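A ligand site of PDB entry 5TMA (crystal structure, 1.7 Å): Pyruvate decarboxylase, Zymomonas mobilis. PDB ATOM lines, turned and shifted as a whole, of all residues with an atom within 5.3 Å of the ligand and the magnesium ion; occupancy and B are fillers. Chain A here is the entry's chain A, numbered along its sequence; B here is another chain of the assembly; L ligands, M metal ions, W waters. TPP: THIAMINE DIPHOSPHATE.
Of the 31 residues printed, 3 come within 4 Å of the magnesium ion. Along chain A the residues within 4 Å of the magnesium ion span positions 440 to 469.
O of Ile 465 lies within hydrogen-bond range of N of Asp 440. OD2 of Asp 440 is in hydrogen-bond range of N of Tyr 468, 3.0 Å away. The side-chain amide nitrogen (ND2) of Asn 467 is in hydrogen-bond range of the side-chain hydroxyl (OG1) of Thr 471 (3.1 Å). The side-chain hydroxyl (OG) of Ser 442 lies within hydrogen-bond range of the backbone carbonyl oxygen (O) of Thr 388 (3.5 Å). OE1 of Glu 473 is in hydrogen-bond range of N of Asp 27 of chain B.
N of Ser 442 lies within hydrogen-bond range of O2A of the ligand (2.8 Å). An oxygen (O2A) of the ligand lies within hydrogen-bond range of the side-chain hydroxyl (OG) of Ser 442 (2.5 Å). The side-chain carboxylate of Glu 50 of chain B is in hydrogen-bond range of a nitrogen (N1') of the ligand, at 2.5 Å. The backbone carbonyl oxygen (O) of Gly 413 lies within hydrogen-bond range of a nitrogen (N4') of the ligand, at 2.6 Å. N of Ile 472 sits at hydrogen-bond distance from O1B of the ligand, 2.7 Å away. N of Asp 390 is in hydrogen-bond range of O3B of the ligand, at 2.8 Å. N of Gly 441 sits close to O1A of the ligand, 2.9 Å away. O1B of the ligand is in hydrogen-bond range of N of Thr 471 (3.2 Å). The backbone NH of Ile 415 sits at hydrogen-bond distance from a nitrogen (N3') of the ligand, 3.0 Å away.
Water W1 lies within hydrogen-bond range of O of Ile 465, ND2 of Asn 467 and N of Asp 440. Water W4 lies within hydrogen-bond range of an oxygen (O2A) of the ligand, the backbone carbonyl oxygen (O) of Thr 388, the backbone NH (N) of Gly 439 and the side-chain hydroxyl (OG) of Ser 442. Water W3 lies within hydrogen-bond range of the side-chain carboxylate (OE2) of Glu 473 (2.7 Å) and the backbone NH (N) of Asp 27 of chain B (3.2 Å). Water W2 lies within hydrogen-bond range of OG of Ser 391 (2.7 Å), O3B of the ligand (3.3 Å) and N of Asp 390 (3.5 Å).
An oxygen (O1A) of the ligand is bound to the magnesium ion, 2.0 Å away. The magnesium ion is bound by O2B of the ligand (2.0 Å). The backbone carbonyl oxygen (O) of Gly 469 binds the magnesium ion (2.1 Å). The side-chain carboxylate (OD1) of Asp 440 is bound to the magnesium ion, at 2.1 Å. Water W1 binds the magnesium ion. The magnesium ion is bound by OD1 of Asn 467, at 2.2 Å. The magnesium ion has six donor atoms within binding distance.
Merely in contact with the ligand: Thr 388 (3.8 Å), Gly 389 (3.7 Å), His 414 (3.3 Å), Gly 439 (3.6 Å), Leu 445 (3.9 Å), Tyr 470 (3.3 Å), Glu 473 (3.6 Å), Ala 25 of chain B (3.3 Å), Gly 26 of chain B (3.5 Å), Thr 72 of chain B (3.98 Å), Val 75 of chain B (3.4 Å) and His 114 of chain B (3.3 Å). Hydrophobic or aromatic side chains that line the ligand: His 414, Ile 415, Leu 445, Tyr 470, Ile 472, Val 75 of chain B and His 114 of chain B. 23 residues have an atom within 4 Å of the ligand: Thr 388, Gly 389, Asp 390, Gly 413, His 414, Ile 415, Gly 439, Asp 440, Gly 441, Ser 442, Leu 445, Asn 467, Gly 469, Tyr 470, Thr 471, Ile 472, Glu 473, Ala 25 of chain B, Gly 26 of chain B, Glu 50 of chain B, Thr 72 of chain B, Val 75 of chain B and His 114 of chain B.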
ATOM      1  N   GLU A 387     -20.529  14.961   3.163  1.00  0.00           N
ATOM      2  CA  GLU A 387     -21.747  14.376   3.745  1.00  0.00           C
ATOM      3  C   GLU A 387     -22.199  13.115   3.008  1.00  0.00           C
ATOM      4  O   GLU A 387     -21.932  12.953   1.792  1.00  0.00           O
ATOM      5  CB  GLU A 387     -22.835  15.419   3.682  1.00  0.00           C
ATOM      6  CG  GLU A 387     -24.135  15.132   4.430  1.00  0.00           C
ATOM      7  CD  GLU A 387     -23.909  14.847   5.881  1.00  0.00           C
ATOM      8  OE1 GLU A 387     -23.536  13.701   6.221  1.00  0.00           O
ATOM      9  OE2 GLU A 387     -24.117  15.713   6.708  1.00  0.00           O
ATOM     10  N   THR A 388     -22.928  12.274   3.784  1.00  0.00           N
ATOM     11  CA  THR A 388     -23.749  11.166   3.249  1.00  0.00           C
ATOM     12  C   THR A 388     -24.754  11.684   2.285  1.00  0.00           C
ATOM     13  O   THR A 388     -25.470  12.615   2.583  1.00  0.00           O
ATOM     14  CB  THR A 388     -24.460  10.411   4.393  1.00  0.00           C
ATOM     15  OG1 THR A 388     -23.442   9.792   5.211  1.00  0.00           O
ATOM     16  CG2 THR A 388     -25.327   9.403   3.839  1.00  0.00           C
ATOM     17  N   GLY A 389     -24.754  11.120   1.099  1.00  0.00           N
ATOM     18  CA  GLY A 389     -25.550  11.687   0.000  1.00  0.00           C
ATOM     19  C   GLY A 389     -24.757  11.489  -1.265  1.00  0.00           C
ATOM     20  O   GLY A 389     -23.693  10.819  -1.261  1.00  0.00           O
ATOM     21  N   ASP A 390     -25.205  12.078  -2.370  1.00  0.00           N
ATOM     22  CA  ASP A 390     -24.329  12.037  -3.577  1.00  0.00           C
ATOM     23  C   ASP A 390     -22.921  12.636  -3.356  1.00  0.00           C
ATOM     24  O   ASP A 390     -22.006  12.243  -4.078  1.00  0.00           O
ATOM     25  CB  ASP A 390     -24.980  12.701  -4.816  1.00  0.00           C
ATOM     26  CG  ASP A 390     -24.498  12.083  -6.138  1.00  0.00           C
ATOM     27  OD1 ASP A 390     -24.008  10.914  -6.132  1.00  0.00           O
ATOM     28  OD2 ASP A 390     -24.573  12.777  -7.188  1.00  0.00           O
ATOM     29  N   SER A 391     -22.729  13.552  -2.357  1.00  0.00           N
ATOM     30  CA  SER A 391     -21.456  14.096  -2.052  1.00  0.00           C
ATOM     31  C   SER A 391     -20.438  13.007  -1.731  1.00  0.00           C
ATOM     32  O   SER A 391     -19.270  13.236  -1.951  1.00  0.00           O
ATOM     33  CB  SER A 391     -21.544  15.090  -0.862  1.00  0.00           C
ATOM     34  OG  SER A 391     -22.240  16.319  -1.224  1.00  0.00           O
ATOM     35  N   GLY A 413     -23.029   7.179   9.161  1.00  0.00           N
ATOM     36  CA  GLY A 413     -23.945   7.687   8.083  1.00  0.00           C
ATOM     37  C   GLY A 413     -25.134   8.497   8.547  1.00  0.00           C
ATOM     38  O   GLY A 413     -26.222   8.299   8.060  1.00  0.00           O
ATOM     39  N   HIS A 414     -24.935   9.396   9.518  1.00  0.00           N
ATOM     40  CA  HIS A 414     -26.018  10.217  10.058  1.00  0.00           C
ATOM     41  C   HIS A 414     -26.100  11.466   9.217  1.00  0.00           C
ATOM     42  O   HIS A 414     -25.206  12.302   9.325  1.00  0.00           O
ATOM     43  CB  HIS A 414     -25.708  10.559  11.510  1.00  0.00           C
ATOM     44  CG  HIS A 414     -26.787  11.277  12.204  1.00  0.00           C
ATOM     45  ND1 HIS A 414     -27.240  12.509  11.790  1.00  0.00           N
ATOM     46  CD2 HIS A 414     -27.446  11.011  13.352  1.00  0.00           C
ATOM     47  CE1 HIS A 414     -28.197  12.918  12.611  1.00  0.00           C
ATOM     48  NE2 HIS A 414     -28.324  12.037  13.566  1.00  0.00           N
ATOM     49  N   ILE A 415     -27.158  11.617   8.414  1.00  0.00           N
ATOM     50  CA  ILE A 415     -27.203  12.801   7.582  1.00  0.00           C
ATOM     51  C   ILE A 415     -27.294  14.002   8.487  1.00  0.00           C
ATOM     52  O   ILE A 415     -27.906  13.980   9.558  1.00  0.00           O
ATOM     53  CB  ILE A 415     -28.303  12.748   6.534  1.00  0.00           C
ATOM     54  CG1 ILE A 415     -29.690  12.574   7.118  1.00  0.00           C
ATOM     55  CG2 ILE A 415     -27.908  11.708   5.480  1.00  0.00           C
ATOM     56  CD1 ILE A 415     -30.802  13.061   6.166  1.00  0.00           C
ATOM     57  N   GLY A 439     -25.506  18.126   1.087  1.00  0.00           N
ATOM     58  CA  GLY A 439     -26.796  18.183   0.420  1.00  0.00           C
ATOM     59  C   GLY A 439     -27.842  18.932   1.221  1.00  0.00           C
ATOM     60  O   GLY A 439     -27.763  19.058   2.458  1.00  0.00           O
ATOM     61  N   ASP A 440     -28.855  19.397   0.505  1.00  0.00           N
ATOM     62  CA  ASP A 440     -29.975  20.148   1.113  1.00  0.00           C
ATOM     63  C   ASP A 440     -30.653  19.387   2.216  1.00  0.00           C
ATOM     64  O   ASP A 440     -30.896  19.941   3.299  1.00  0.00           O
ATOM     65  CB  ASP A 440     -30.939  20.651   0.051  1.00  0.00           C
ATOM     66  CG  ASP A 440     -31.553  19.482  -0.829  1.00  0.00           C
ATOM     67  OD1 ASP A 440     -30.904  18.412  -1.054  1.00  0.00           O
ATOM     68  OD2 ASP A 440     -32.708  19.608  -1.270  1.00  0.00           O
ATOM     69  N   GLY A 441     -31.001  18.124   1.983  1.00  0.00           N
ATOM     70  CA  GLY A 441     -31.645  17.273   2.991  1.00  0.00           C
ATOM     71  C   GLY A 441     -30.925  17.085   4.274  1.00  0.00           C
ATOM     72  O   GLY A 441     -31.493  17.268   5.355  1.00  0.00           O
ATOM     73  N   SER A 442     -29.668  16.775   4.159  1.00  0.00           N
ATOM     74  CA  SER A 442     -28.760  16.688   5.301  1.00  0.00           C
ATOM     75  C   SER A 442     -28.621  17.984   6.034  1.00  0.00           C
ATOM     76  O   SER A 442     -28.676  17.993   7.273  1.00  0.00           O
ATOM     77  CB  SER A 442     -27.379  16.246   4.836  1.00  0.00           C
ATOM     78  OG  SER A 442     -27.469  14.914   4.288  1.00  0.00           O
ATOM     79  N   PHE A 443     -28.470  19.077   5.274  1.00  0.00           N
ATOM     80  CA  PHE A 443     -28.211  20.372   5.865  1.00  0.00           C
ATOM     81  C   PHE A 443     -29.323  20.707   6.837  1.00  0.00           C
ATOM     82  O   PHE A 443     -29.074  21.284   7.876  1.00  0.00           O
ATOM     83  CB  PHE A 443     -28.096  21.449   4.769  1.00  0.00           C
ATOM     84  CG  PHE A 443     -27.684  22.770   5.267  1.00  0.00           C
ATOM     85  CD1 PHE A 443     -26.409  23.060   5.582  1.00  0.00           C
ATOM     86  CD2 PHE A 443     -28.647  23.751   5.373  1.00  0.00           C
ATOM     87  CE1 PHE A 443     -26.091  24.364   5.992  1.00  0.00           C
ATOM     88  CE2 PHE A 443     -28.350  25.033   5.791  1.00  0.00           C
ATOM     89  CZ  PHE A 443     -27.061  25.333   6.133  1.00  0.00           C
ATOM     90  N   LEU A 445     -31.001  19.033   8.958  1.00  0.00           N
ATOM     91  CA  LEU A 445     -30.997  18.396  10.283  1.00  0.00           C
ATOM     92  C   LEU A 445     -30.214  19.155  11.346  1.00  0.00           C
ATOM     93  O   LEU A 445     -30.520  19.053  12.552  1.00  0.00           O
ATOM     94  CB  LEU A 445     -30.477  16.957  10.204  1.00  0.00           C
ATOM     95  CG  LEU A 445     -31.470  15.912   9.707  1.00  0.00           C
ATOM     96  CD1 LEU A 445     -31.305  15.768   8.210  1.00  0.00           C
ATOM     97  CD2 LEU A 445     -31.187  14.579  10.393  1.00  0.00           C
ATOM     98  N   ILE A 465     -25.623  21.605  -1.906  1.00  0.00           N
ATOM     99  CA  ILE A 465     -26.120  21.057  -3.196  1.00  0.00           C
ATOM    100  C   ILE A 465     -27.611  20.978  -3.129  1.00  0.00           C
ATOM    101  O   ILE A 465     -28.187  20.082  -2.442  1.00  0.00           O
ATOM    102  CB  ILE A 465     -25.503  19.679  -3.489  1.00  0.00           C
ATOM    103  CG1 ILE A 465     -23.998  19.726  -3.279  1.00  0.00           C
ATOM    104  CG2 ILE A 465     -25.933  19.213  -4.876  1.00  0.00           C
ATOM    105  CD1 ILE A 465     -23.248  20.728  -4.046  1.00  0.00           C
ATOM    106  N   ASN A 467     -30.583  19.976  -4.686  1.00  0.00           N
ATOM    107  CA  ASN A 467     -31.288  19.091  -5.646  1.00  0.00           C
ATOM    108  C   ASN A 467     -32.713  18.694  -5.138  1.00  0.00           C
ATOM    109  O   ASN A 467     -33.264  17.664  -5.523  1.00  0.00           O
ATOM    110  CB  ASN A 467     -30.413  17.842  -5.970  1.00  0.00           C
ATOM    111  CG  ASN A 467     -30.188  16.959  -4.782  1.00  0.00           C
ATOM    112  OD1 ASN A 467     -30.820  17.164  -3.735  1.00  0.00           O
ATOM    113  ND2 ASN A 467     -29.346  15.926  -4.934  1.00  0.00           N
ATOM    114  N   TYR A 468     -33.306  19.498  -4.244  1.00  0.00           N
ATOM    115  CA  TYR A 468     -34.721  19.389  -3.881  1.00  0.00           C
ATOM    116  C   TYR A 468     -35.111  18.000  -3.354  1.00  0.00           C
ATOM    117  O   TYR A 468     -36.038  17.362  -3.845  1.00  0.00           O
ATOM    118  CB  TYR A 468     -35.622  19.813  -5.066  1.00  0.00           C
ATOM    119  CG  TYR A 468     -35.281  21.209  -5.586  1.00  0.00           C
ATOM    120  CD1 TYR A 468     -35.844  22.356  -4.979  1.00  0.00           C
ATOM    121  CD2 TYR A 468     -34.387  21.417  -6.657  1.00  0.00           C
ATOM    122  CE1 TYR A 468     -35.552  23.642  -5.412  1.00  0.00           C
ATOM    123  CE2 TYR A 468     -34.092  22.715  -7.111  1.00  0.00           C
ATOM    124  CZ  TYR A 468     -34.685  23.822  -6.470  1.00  0.00           C
ATOM    125  OH  TYR A 468     -34.408  25.102  -6.907  1.00  0.00           O
ATOM    126  N   GLY A 469     -34.347  17.530  -2.373  1.00  0.00           N
ATOM    127  CA  GLY A 469     -34.697  16.334  -1.579  1.00  0.00           C
ATOM    128  C   GLY A 469     -33.588  15.292  -1.399  1.00  0.00           C
ATOM    129  O   GLY A 469     -32.391  15.595  -1.602  1.00  0.00           O
ATOM    130  N   TYR A 470     -34.001  14.054  -1.054  1.00  0.00           N
ATOM    131  CA  TYR A 470     -33.025  13.028  -0.641  1.00  0.00           C
ATOM    132  C   TYR A 470     -32.686  12.123  -1.856  1.00  0.00           C
ATOM    133  O   TYR A 470     -33.285  11.023  -2.036  1.00  0.00           O
ATOM    134  CB  TYR A 470     -33.628  12.104   0.430  1.00  0.00           C
ATOM    135  CG  TYR A 470     -34.068  12.762   1.714  1.00  0.00           C
ATOM    136  CD1 TYR A 470     -33.354  13.797   2.326  1.00  0.00           C
ATOM    137  CD2 TYR A 470     -35.118  12.177   2.450  1.00  0.00           C
ATOM    138  CE1 TYR A 470     -33.732  14.310   3.582  1.00  0.00           C
ATOM    139  CE2 TYR A 470     -35.550  12.705   3.660  1.00  0.00           C
ATOM    140  CZ  TYR A 470     -34.865  13.771   4.234  1.00  0.00           C
ATOM    141  OH  TYR A 470     -35.290  14.296   5.506  1.00  0.00           O
ATOM    142  N   THR A 471     -31.794  12.607  -2.694  1.00  0.00           N
ATOM    143  CA  THR A 471     -31.559  11.939  -3.980  1.00  0.00           C
ATOM    144  C   THR A 471     -30.954  10.552  -3.797  1.00  0.00           C
ATOM    145  O   THR A 471     -31.327   9.616  -4.489  1.00  0.00           O
ATOM    146  CB  THR A 471     -30.795  12.894  -4.928  1.00  0.00           C
ATOM    147  OG1 THR A 471     -31.717  13.930  -5.362  1.00  0.00           O
ATOM    148  CG2 THR A 471     -30.198  12.147  -6.182  1.00  0.00           C
ATOM    149  N   ILE A 472     -30.009  10.396  -2.888  1.00  0.00           N
ATOM    150  CA  ILE A 472     -29.535   9.004  -2.581  1.00  0.00           C
ATOM    151  C   ILE A 472     -30.703   7.991  -2.229  1.00  0.00           C
ATOM    152  O   ILE A 472     -30.727   6.869  -2.739  1.00  0.00           O
ATOM    153  CB  ILE A 472     -28.446   9.074  -1.492  1.00  0.00           C
ATOM    154  CG1 ILE A 472     -27.773   7.739  -1.213  1.00  0.00           C
ATOM    155  CG2 ILE A 472     -29.034   9.628  -0.210  1.00  0.00           C
ATOM    156  CD1 ILE A 472     -26.479   7.914  -0.407  1.00  0.00           C
ATOM    157  N   GLU A 473     -31.697   8.430  -1.419  1.00  0.00           N
ATOM    158  CA  GLU A 473     -32.853   7.556  -1.090  1.00  0.00           C
ATOM    159  C   GLU A 473     -33.675   7.331  -2.353  1.00  0.00           C
ATOM    160  O   GLU A 473     -34.241   6.220  -2.545  1.00  0.00           O
ATOM    161  CB  GLU A 473     -33.782   8.128   0.009  1.00  0.00           C
ATOM    162  CG  GLU A 473     -33.121   8.508   1.308  1.00  0.00           C
ATOM    163  CD  GLU A 473     -32.565   7.314   2.027  1.00  0.00           C
ATOM    164  OE1 GLU A 473     -33.250   6.884   2.935  1.00  0.00           O
ATOM    165  OE2 GLU A 473     -31.478   6.811   1.680  1.00  0.00           O
ATOM    166  N   VAL B  24     -39.158  10.103   9.657  1.00  0.00           N
ATOM    167  CA  VAL B  24     -37.990  10.471   8.864  1.00  0.00           C
ATOM    168  C   VAL B  24     -37.543   9.204   8.183  1.00  0.00           C
ATOM    169  O   VAL B  24     -37.241   8.202   8.814  1.00  0.00           O
ATOM    170  CB  VAL B  24     -36.829  11.042   9.734  1.00  0.00           C
ATOM    171  CG1 VAL B  24     -35.671  11.443   8.835  1.00  0.00           C
ATOM    172  CG2 VAL B  24     -37.328  12.197  10.552  1.00  0.00           C
ATOM    173  N   ALA B  25     -37.476   9.278   6.860  1.00  0.00           N
ATOM    174  CA  ALA B  25     -37.021   8.148   6.036  1.00  0.00           C
ATOM    175  C   ALA B  25     -35.583   7.754   6.202  1.00  0.00           C
ATOM    176  O   ALA B  25     -34.681   8.575   6.379  1.00  0.00           O
ATOM    177  CB  ALA B  25     -37.196   8.495   4.580  1.00  0.00           C
ATOM    178  N   GLY B  26     -35.349   6.484   6.033  1.00  0.00           N
ATOM    179  CA  GLY B  26     -34.012   5.936   5.885  1.00  0.00           C
ATOM    180  C   GLY B  26     -34.091   4.534   5.331  1.00  0.00           C
ATOM    181  O   GLY B  26     -35.165   3.851   5.364  1.00  0.00           O
ATOM    182  N   ASP B  27     -33.002   4.054   4.770  1.00  0.00           N
ATOM    183  CA  ASP B  27     -33.124   2.769   4.050  1.00  0.00           C
ATOM    184  C   ASP B  27     -33.653   1.550   4.856  1.00  0.00           C
ATOM    185  O   ASP B  27     -34.408   0.730   4.258  1.00  0.00           O
ATOM    186  CB  ASP B  27     -31.906   2.473   3.185  1.00  0.00           C
ATOM    187  CG  ASP B  27     -30.705   2.149   3.968  1.00  0.00           C
ATOM    188  OD1 ASP B  27     -30.714   2.482   5.175  1.00  0.00           O
ATOM    189  OD2 ASP B  27     -29.733   1.553   3.391  1.00  0.00           O
ATOM    190  N   GLU B  50     -34.769  13.623  13.654  1.00  0.00           N
ATOM    191  CA  GLU B  50     -35.407  12.655  14.492  1.00  0.00           C
ATOM    192  C   GLU B  50     -35.712  13.102  15.908  1.00  0.00           C
ATOM    193  O   GLU B  50     -36.744  12.655  16.461  1.00  0.00           O
ATOM    194  CB  GLU B  50     -34.632  11.342  14.521  1.00  0.00           C
ATOM    195  CG  GLU B  50     -34.666  10.652  13.146  1.00  0.00           C
ATOM    196  CD  GLU B  50     -33.510  11.094  12.232  1.00  0.00           C
ATOM    197  OE1 GLU B  50     -32.707  12.075  12.611  1.00  0.00           O
ATOM    198  OE2 GLU B  50     -33.419  10.403  11.108  1.00  0.00           O
ATOM    199  N   THR B  72     -35.303   5.633  11.369  1.00  0.00           N
ATOM    200  CA  THR B  72     -34.344   4.623  10.914  1.00  0.00           C
ATOM    201  C   THR B  72     -33.360   4.193  12.021  1.00  0.00           C
ATOM    202  O   THR B  72     -33.060   4.874  12.989  1.00  0.00           O
ATOM    203  CB  THR B  72     -33.545   4.947   9.580  1.00  0.00           C
ATOM    204  OG1 THR B  72     -33.193   3.683   8.922  1.00  0.00           O
ATOM    205  CG2 THR B  72     -32.285   5.862   9.874  1.00  0.00           C
ATOM    206  N   VAL B  75     -28.964   5.696  13.786  1.00  0.00           N
ATOM    207  CA  VAL B  75     -28.860   7.145  13.551  1.00  0.00           C
ATOM    208  C   VAL B  75     -30.189   7.915  13.794  1.00  0.00           C
ATOM    209  O   VAL B  75     -30.207   9.066  14.159  1.00  0.00           O
ATOM    210  CB  VAL B  75     -28.283   7.445  12.143  1.00  0.00           C
ATOM    211  CG1 VAL B  75     -26.909   6.852  12.064  1.00  0.00           C
ATOM    212  CG2 VAL B  75     -29.153   6.870  11.028  1.00  0.00           C
ATOM    213  N   GLY B  76     -31.328   7.302  13.514  1.00  0.00           N
ATOM    214  CA  GLY B  76     -32.579   7.987  13.794  1.00  0.00           C
ATOM    215  C   GLY B  76     -33.044   7.747  15.207  1.00  0.00           C
ATOM    216  O   GLY B  76     -33.496   8.650  15.887  1.00  0.00           O
ATOM    217  N   HIS B 114     -24.933   2.358   9.621  1.00  0.00           N
ATOM    218  CA  HIS B 114     -25.707   2.976  10.723  1.00  0.00           C
ATOM    219  C   HIS B 114     -25.441   2.391  12.106  1.00  0.00           C
ATOM    220  O   HIS B 114     -25.810   2.911  13.120  1.00  0.00           O
ATOM    221  CB  HIS B 114     -27.207   3.011  10.494  1.00  0.00           C
ATOM    222  CG  HIS B 114     -27.679   3.890   9.373  1.00  0.00           C
ATOM    223  ND1 HIS B 114     -26.890   4.817   8.720  1.00  0.00           N
ATOM    224  CD2 HIS B 114     -28.916   4.051   8.857  1.00  0.00           C
ATOM    225  CE1 HIS B 114     -27.606   5.473   7.824  1.00  0.00           C
ATOM    226  NE2 HIS B 114     -28.836   5.009   7.873  1.00  0.00           N
HETATM  227  N1' TPP L   1     -31.727  10.027   9.276  1.00  0.00           N
HETATM  228  C2' TPP L   1     -30.397  10.116   9.663  1.00  0.00           C
HETATM  229  CM2 TPP L   1     -30.183  10.849  10.901  1.00  0.00           C
HETATM  230  N3' TPP L   1     -29.368   9.631   8.973  1.00  0.00           N
HETATM  231  C4' TPP L   1     -29.619   9.006   7.806  1.00  0.00           C
HETATM  232  N4' TPP L   1     -28.611   8.498   7.125  1.00  0.00           N
HETATM  233  C5' TPP L   1     -31.008   8.883   7.298  1.00  0.00           C
HETATM  234  C6' TPP L   1     -32.017   9.416   8.098  1.00  0.00           C
HETATM  235  C7' TPP L   1     -31.280   8.190   5.961  1.00  0.00           C
HETATM  236  N3  TPP L   1     -30.649   8.855   4.798  1.00  0.00           N
HETATM  237  C2  TPP L   1     -29.486   8.480   4.136  1.00  0.00           C
HETATM  238  S1  TPP L   1     -28.965   9.509   2.770  1.00  0.00           S
HETATM  239  C5  TPP L   1     -30.445  10.441   3.030  1.00  0.00           C
HETATM  240  C4  TPP L   1     -31.259   9.933   4.171  1.00  0.00           C
HETATM  241  CM4 TPP L   1     -32.581  10.558   4.621  1.00  0.00           C
HETATM  242  C6  TPP L   1     -30.652  11.587   2.105  1.00  0.00           C
HETATM  243  C7  TPP L   1     -29.640  12.738   2.181  1.00  0.00           C
HETATM  244  O7  TPP L   1     -30.170  13.750   1.318  1.00  0.00           O
HETATM  245  PA  TPP L   1     -29.246  14.997   0.823  1.00  0.00           P
HETATM  246  O1A TPP L   1     -30.140  16.031   0.236  1.00  0.00           O
HETATM  247  O2A TPP L   1     -28.399  15.418   2.047  1.00  0.00           O
HETATM  248  O3A TPP L   1     -28.159  14.357  -0.185  1.00  0.00           O
HETATM  249  PB  TPP L   1     -28.549  13.876  -1.707  1.00  0.00           P
HETATM  250  O1B TPP L   1     -28.822  12.382  -1.472  1.00  0.00           O
HETATM  251  O2B TPP L   1     -29.754  14.603  -2.255  1.00  0.00           O
HETATM  252  O3B TPP L   1     -27.302  13.935  -2.498  1.00  0.00           O
HETATM  253 MG    MG M   1     -30.488  16.422  -1.686  1.00  0.00          MG
HETATM  254  O   HOH W   1     -28.530  17.276  -2.121  1.00  0.00           O
HETATM  255  O   HOH W   2     -24.707  15.231  -1.005  1.00  0.00           O
HETATM  256  O   HOH W   3     -30.328   5.363   3.710  1.00  0.00           O
HETATM  257  O   HOH W   4     -25.803  15.261   1.546  1.00  0.00           O
